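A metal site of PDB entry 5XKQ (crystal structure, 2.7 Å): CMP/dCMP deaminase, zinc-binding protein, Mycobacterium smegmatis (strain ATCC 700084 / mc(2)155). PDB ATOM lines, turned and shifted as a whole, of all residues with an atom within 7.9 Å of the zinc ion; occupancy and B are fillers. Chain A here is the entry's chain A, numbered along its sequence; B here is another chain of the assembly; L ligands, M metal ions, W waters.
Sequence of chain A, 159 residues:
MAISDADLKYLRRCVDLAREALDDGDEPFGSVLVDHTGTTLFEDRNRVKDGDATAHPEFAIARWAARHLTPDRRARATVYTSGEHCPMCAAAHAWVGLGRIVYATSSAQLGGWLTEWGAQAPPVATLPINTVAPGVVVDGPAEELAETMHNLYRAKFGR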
ATOM      1  N   PHE A  29      29.263 -33.020 -22.154  1.00  0.00           N
ATOM      2  CA  PHE A  29      27.932 -32.743 -22.684  1.00  0.00           C
ATOM      3  C   PHE A  29      27.354 -34.016 -23.287  1.00  0.00           C
ATOM      4  O   PHE A  29      28.019 -34.706 -24.068  1.00  0.00           O
ATOM      5  CB  PHE A  29      28.009 -31.696 -23.786  1.00  0.00           C
ATOM      6  CG  PHE A  29      28.454 -30.351 -23.326  1.00  0.00           C
ATOM      7  CD1 PHE A  29      27.537 -29.435 -22.841  1.00  0.00           C
ATOM      8  CD2 PHE A  29      29.794 -29.975 -23.430  1.00  0.00           C
ATOM      9  CE1 PHE A  29      27.953 -28.173 -22.448  1.00  0.00           C
ATOM     10  CE2 PHE A  29      30.211 -28.713 -23.036  1.00  0.00           C
ATOM     11  CZ  PHE A  29      29.287 -27.813 -22.537  1.00  0.00           C
ATOM     12  N   ASN A  46      29.647 -35.217 -26.696  1.00  0.00           N
ATOM     13  CA  ASN A  46      30.617 -34.337 -27.348  1.00  0.00           C
ATOM     14  C   ASN A  46      31.785 -35.105 -27.992  1.00  0.00           C
ATOM     15  O   ASN A  46      32.184 -36.165 -27.509  1.00  0.00           O
ATOM     16  CB  ASN A  46      31.146 -33.362 -26.307  1.00  0.00           C
ATOM     17  CG  ASN A  46      32.101 -32.347 -26.893  1.00  0.00           C
ATOM     18  OD1 ASN A  46      33.301 -32.633 -27.033  1.00  0.00           O
ATOM     19  ND2 ASN A  46      31.588 -31.154 -27.214  1.00  0.00           N
ATOM     20  N   ALA A  53      34.913 -28.282 -33.959  1.00  0.00           N
ATOM     21  CA  ALA A  53      34.241 -27.564 -32.836  1.00  0.00           C
ATOM     22  C   ALA A  53      32.676 -27.498 -32.835  1.00  0.00           C
ATOM     23  O   ALA A  53      32.078 -27.118 -31.821  1.00  0.00           O
ATOM     24  CB  ALA A  53      34.835 -26.159 -32.710  1.00  0.00           C
ATOM     25  N   THR A  54      32.042 -27.866 -33.956  1.00  0.00           N
ATOM     26  CA  THR A  54      30.572 -27.985 -34.042  1.00  0.00           C
ATOM     27  C   THR A  54      30.002 -29.384 -33.671  1.00  0.00           C
ATOM     28  O   THR A  54      28.797 -29.632 -33.823  1.00  0.00           O
ATOM     29  CB  THR A  54      30.083 -27.625 -35.478  1.00  0.00           C
ATOM     30  OG1 THR A  54      30.370 -28.700 -36.389  1.00  0.00           O
ATOM     31  CG2 THR A  54      30.721 -26.310 -35.987  1.00  0.00           C
ATOM     32  N   ALA A  55      30.852 -30.310 -33.188  1.00  0.00           N
ATOM     33  CA  ALA A  55      30.454 -31.706 -32.889  1.00  0.00           C
ATOM     34  C   ALA A  55      29.701 -31.815 -31.531  1.00  0.00           C
ATOM     35  O   ALA A  55      30.159 -32.446 -30.581  1.00  0.00           O
ATOM     36  CB  ALA A  55      31.673 -32.610 -32.883  1.00  0.00           C
ATOM     37  N   HIS A  56      28.532 -31.168 -31.488  1.00  0.00           N
ATOM     38  CA  HIS A  56      27.722 -31.041 -30.285  1.00  0.00           C
ATOM     39  C   HIS A  56      26.655 -32.104 -30.396  1.00  0.00           C
ATOM     40  O   HIS A  56      26.067 -32.268 -31.456  1.00  0.00           O
ATOM     41  CB  HIS A  56      27.063 -29.657 -30.223  1.00  0.00           C
ATOM     42  CG  HIS A  56      28.008 -28.525 -29.953  1.00  0.00           C
ATOM     43  ND1 HIS A  56      27.601 -27.300 -29.454  1.00  0.00           N
ATOM     44  CD2 HIS A  56      29.360 -28.454 -30.074  1.00  0.00           C
ATOM     45  CE1 HIS A  56      28.664 -26.529 -29.290  1.00  0.00           C
ATOM     46  NE2 HIS A  56      29.734 -27.201 -29.656  1.00  0.00           N
ATOM     47  N   PRO A  57      26.373 -32.829 -29.307  1.00  0.00           N
ATOM     48  CA  PRO A  57      25.426 -33.939 -29.417  1.00  0.00           C
ATOM     49  C   PRO A  57      24.018 -33.508 -29.792  1.00  0.00           C
ATOM     50  O   PRO A  57      23.305 -34.280 -30.425  1.00  0.00           O
ATOM     51  CB  PRO A  57      25.454 -34.598 -28.036  1.00  0.00           C
ATOM     52  CG  PRO A  57      26.028 -33.573 -27.122  1.00  0.00           C
ATOM     53  CD  PRO A  57      26.926 -32.702 -27.957  1.00  0.00           C
ATOM     54  N   GLU A  58      23.635 -32.287 -29.428  1.00  0.00           N
ATOM     55  CA  GLU A  58      22.315 -31.765 -29.761  1.00  0.00           C
ATOM     56  C   GLU A  58      22.208 -31.538 -31.264  1.00  0.00           C
ATOM     57  O   GLU A  58      21.156 -31.760 -31.865  1.00  0.00           O
ATOM     58  CB  GLU A  58      22.073 -30.445 -29.042  1.00  0.00           C
ATOM     59  CG  GLU A  58      22.187 -30.510 -27.530  1.00  0.00           C
ATOM     60  CD  GLU A  58      23.565 -30.163 -26.983  1.00  0.00           C
ATOM     61  OE1 GLU A  58      24.601 -30.394 -27.666  1.00  0.00           O
ATOM     62  OE2 GLU A  58      23.608 -29.641 -25.850  1.00  0.00           O
ATOM     63  N   PHE A  59      23.302 -31.108 -31.883  1.00  0.00           N
ATOM     64  CA  PHE A  59      23.324 -30.871 -33.324  1.00  0.00           C
ATOM     65  C   PHE A  59      23.287 -32.220 -34.027  1.00  0.00           C
ATOM     66  O   PHE A  59      22.497 -32.417 -34.942  1.00  0.00           O
ATOM     67  CB  PHE A  59      24.572 -30.106 -33.763  1.00  0.00           C
ATOM     68  CG  PHE A  59      24.520 -29.671 -35.174  1.00  0.00           C
ATOM     69  CD1 PHE A  59      23.781 -28.559 -35.531  1.00  0.00           C
ATOM     70  CD2 PHE A  59      25.154 -30.419 -36.171  1.00  0.00           C
ATOM     71  CE1 PHE A  59      23.681 -28.162 -36.860  1.00  0.00           C
ATOM     72  CE2 PHE A  59      25.061 -30.028 -37.504  1.00  0.00           C
ATOM     73  CZ  PHE A  59      24.327 -28.903 -37.851  1.00  0.00           C
ATOM     74  N   GLY A  83      23.220 -30.069 -20.655  1.00  0.00           N
ATOM     75  CA  GLY A  83      23.412 -28.619 -20.663  1.00  0.00           C
ATOM     76  C   GLY A  83      22.603 -27.979 -21.761  1.00  0.00           C
ATOM     77  O   GLY A  83      22.650 -28.425 -22.892  1.00  0.00           O
ATOM     78  N   GLU A  84      21.869 -26.920 -21.428  1.00  0.00           N
ATOM     79  CA  GLU A  84      21.033 -26.190 -22.389  1.00  0.00           C
ATOM     80  C   GLU A  84      21.716 -25.917 -23.726  1.00  0.00           C
ATOM     81  O   GLU A  84      22.857 -25.508 -23.759  1.00  0.00           O
ATOM     82  CB  GLU A  84      20.584 -24.848 -21.787  1.00  0.00           C
ATOM     83  CG  GLU A  84      19.843 -23.893 -22.737  1.00  0.00           C
ATOM     84  CD  GLU A  84      19.188 -22.734 -21.999  1.00  0.00           C
ATOM     85  OE1 GLU A  84      19.689 -22.312 -20.928  1.00  0.00           O
ATOM     86  OE2 GLU A  84      18.173 -22.227 -22.512  1.00  0.00           O
ATOM     87  N   HIS A  85      20.988 -26.123 -24.812  1.00  0.00           N
ATOM     88  CA  HIS A  85      21.515 -26.008 -26.158  1.00  0.00           C
ATOM     89  C   HIS A  85      22.172 -24.642 -26.350  1.00  0.00           C
ATOM     90  O   HIS A  85      21.560 -23.649 -25.985  1.00  0.00           O
ATOM     91  CB  HIS A  85      20.362 -26.077 -27.195  1.00  0.00           C
ATOM     92  CG  HIS A  85      19.704 -27.412 -27.353  1.00  0.00           C
ATOM     93  ND1 HIS A  85      19.209 -28.146 -26.299  1.00  0.00           N
ATOM     94  CD2 HIS A  85      19.386 -28.105 -28.472  1.00  0.00           C
ATOM     95  CE1 HIS A  85      18.663 -29.267 -26.757  1.00  0.00           C
ATOM     96  NE2 HIS A  85      18.755 -29.263 -28.074  1.00  0.00           N
ATOM     97  N   CYS A  86      23.355 -24.587 -26.963  1.00  0.00           N
ATOM     98  CA  CYS A  86      23.898 -23.326 -27.468  1.00  0.00           C
ATOM     99  C   CYS A  86      23.053 -22.843 -28.663  1.00  0.00           C
ATOM    100  O   CYS A  86      22.218 -23.599 -29.171  1.00  0.00           O
ATOM    101  CB  CYS A  86      25.368 -23.484 -27.888  1.00  0.00           C
ATOM    102  SG  CYS A  86      25.643 -24.246 -29.507  1.00  0.00           S
ATOM    103  N   PRO A  87      23.257 -21.600 -29.114  1.00  0.00           N
ATOM    104  CA  PRO A  87      22.480 -21.064 -30.236  1.00  0.00           C
ATOM    105  C   PRO A  87      22.498 -21.866 -31.533  1.00  0.00           C
ATOM    106  O   PRO A  87      21.479 -21.903 -32.257  1.00  0.00           O
ATOM    107  CB  PRO A  87      23.098 -19.687 -30.450  1.00  0.00           C
ATOM    108  CG  PRO A  87      23.441 -19.272 -29.068  1.00  0.00           C
ATOM    109  CD  PRO A  87      23.918 -20.520 -28.366  1.00  0.00           C
ATOM    110  N   MET A  88      23.638 -22.455 -31.847  1.00  0.00           N
ATOM    111  CA  MET A  88      23.759 -23.372 -33.000  1.00  0.00           C
ATOM    112  C   MET A  88      22.776 -24.542 -32.918  1.00  0.00           C
ATOM    113  O   MET A  88      22.031 -24.810 -33.849  1.00  0.00           O
ATOM    114  CB  MET A  88      25.167 -23.919 -33.107  1.00  0.00           C
ATOM    115  CG  MET A  88      25.460 -24.652 -34.399  1.00  0.00           C
ATOM    116  SD  MET A  88      27.157 -25.245 -34.443  1.00  0.00           S
ATOM    117  CE  MET A  88      26.932 -26.564 -33.241  1.00  0.00           C
ATOM    118  N   CYS A  89      22.776 -25.212 -31.771  1.00  0.00           N
ATOM    119  CA  CYS A  89      21.959 -26.407 -31.596  1.00  0.00           C
ATOM    120  C   CYS A  89      20.508 -26.042 -31.454  1.00  0.00           C
ATOM    121  O   CYS A  89      19.658 -26.746 -31.968  1.00  0.00           O
ATOM    122  CB  CYS A  89      22.431 -27.194 -30.381  1.00  0.00           C
ATOM    123  SG  CYS A  89      24.136 -27.804 -30.563  1.00  0.00           S
ATOM    124  N   ALA A  90      20.235 -24.944 -30.773  1.00  0.00           N
ATOM    125  CA  ALA A  90      18.865 -24.476 -30.572  1.00  0.00           C
ATOM    126  C   ALA A  90      18.231 -24.126 -31.894  1.00  0.00           C
ATOM    127  O   ALA A  90      17.053 -24.413 -32.128  1.00  0.00           O
ATOM    128  CB  ALA A  90      18.855 -23.284 -29.636  1.00  0.00           C
ATOM    129  N   VAL A 124      30.573 -17.785 -28.653  1.00  0.00           N
ATOM    130  CA  VAL A 124      29.138 -17.736 -28.831  1.00  0.00           C
ATOM    131  C   VAL A 124      28.457 -17.400 -27.511  1.00  0.00           C
ATOM    132  O   VAL A 124      28.697 -18.053 -26.499  1.00  0.00           O
ATOM    133  CB  VAL A 124      28.601 -19.104 -29.308  1.00  0.00           C
ATOM    134  CG1 VAL A 124      27.091 -19.070 -29.405  1.00  0.00           C
ATOM    135  CG2 VAL A 124      29.213 -19.462 -30.660  1.00  0.00           C
ATOM    136  N   ALA B  91      26.607 -18.903 -35.117  1.00  0.00           N
ATOM    137  CA  ALA B  91      27.247 -19.594 -34.028  1.00  0.00           C
ATOM    138  C   ALA B  91      28.315 -20.531 -34.551  1.00  0.00           C
ATOM    139  O   ALA B  91      29.404 -20.582 -34.004  1.00  0.00           O
ATOM    140  CB  ALA B  91      26.222 -20.362 -33.241  1.00  0.00           C
ATOM    141  N   TRP B  95      32.250 -20.628 -33.602  1.00  0.00           N
ATOM    142  CA  TRP B  95      32.856 -21.813 -32.982  1.00  0.00           C
ATOM    143  C   TRP B  95      34.106 -22.331 -33.758  1.00  0.00           C
ATOM    144  O   TRP B  95      35.087 -22.706 -33.156  1.00  0.00           O
ATOM    145  CB  TRP B  95      31.865 -22.965 -32.869  1.00  0.00           C
ATOM    146  CG  TRP B  95      30.841 -22.879 -31.788  1.00  0.00           C
ATOM    147  CD1 TRP B  95      29.488 -22.921 -31.947  1.00  0.00           C
ATOM    148  CD2 TRP B  95      31.071 -22.784 -30.384  1.00  0.00           C
ATOM    149  NE1 TRP B  95      28.860 -22.851 -30.736  1.00  0.00           N
ATOM    150  CE2 TRP B  95      29.805 -22.732 -29.751  1.00  0.00           C
ATOM    151  CE3 TRP B  95      32.239 -22.712 -29.593  1.00  0.00           C
ATOM    152  CZ2 TRP B  95      29.654 -22.630 -28.358  1.00  0.00           C
ATOM    153  CZ3 TRP B  95      32.089 -22.601 -28.211  1.00  0.00           C
ATOM    154  CH2 TRP B  95      30.812 -22.566 -27.610  1.00  0.00           C
HETATM  155  O1  LIG L   1      28.850 -29.632 -26.925  1.00  0.00           O
HETATM  156  C1  LIG L   1      28.819 -28.365 -26.513  1.00  0.00           C
HETATM  157  N1  LIG L   1      29.979 -27.720 -26.391  1.00  0.00           N
HETATM  158  N2  LIG L   1      27.634 -27.825 -26.249  1.00  0.00           N
HETATM  159  C2  LIG L   1      27.628 -26.523 -25.836  1.00  0.00           C
HETATM  160  N3  LIG L   1      26.442 -25.958 -25.544  1.00  0.00           N
HETATM  161  N4  LIG L   1      28.754 -25.795 -25.681  1.00  0.00           N
HETATM  162  C3  LIG L   1      29.916 -26.409 -25.976  1.00  0.00           C
HETATM  163  N5  LIG L   1      31.064 -25.736 -25.843  1.00  0.00           N
HETATM  164 ZN    ZN M   1      25.606 -26.546 -29.259  1.00  0.00          ZN
HETATM  165  O   HOH W   1      24.710 -27.096 -27.546  1.00  0.00           O
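Water W1 lies within hydrogen-bond range of a nitrogen (N3) of the ligand (2.9 Å), the backbone NH of Cys 86 (2.9 Å) and the side-chain carboxylate of Glu 58 (3.3 Å).
The zinc ion is bound by water W1.
The zinc ion is bound by ND1 of His 56 (2.1 Å).
The side-chain sulfur (SG) of Cys 86 is bound to the zinc ion (2.3 Å).
The zinc ion is bound by SG of Cys 89 (2.3 Å).
The zinc ion has four donor atoms within binding distance.
A ring nitrogen (NE2) of His 56 lies within hydrogen-bond range of a nitrogen (N1) of the ligand, at 3.3 Å.
The side-chain amide nitrogen of Asn 46 is in hydrogen-bond range of an oxygen (O1) of the ligand, at 3.1 Å.
NE2 of His 56 is in hydrogen-bond range of O of Ala 53, at 3.2 Å.
SG of Cys 86 lies close to N of Met 88, 3.6 Å away.
SG of Cys 86 lies close to NE1 of Trp 95 of chain B.
The side-chain sulfur (SG) of Cys 89 lies close to the backbone NH (N) of Phe 59, at 3.7 Å.
Within 4 Å of the zinc ion: His 56, Cys 86 and Cys 89.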
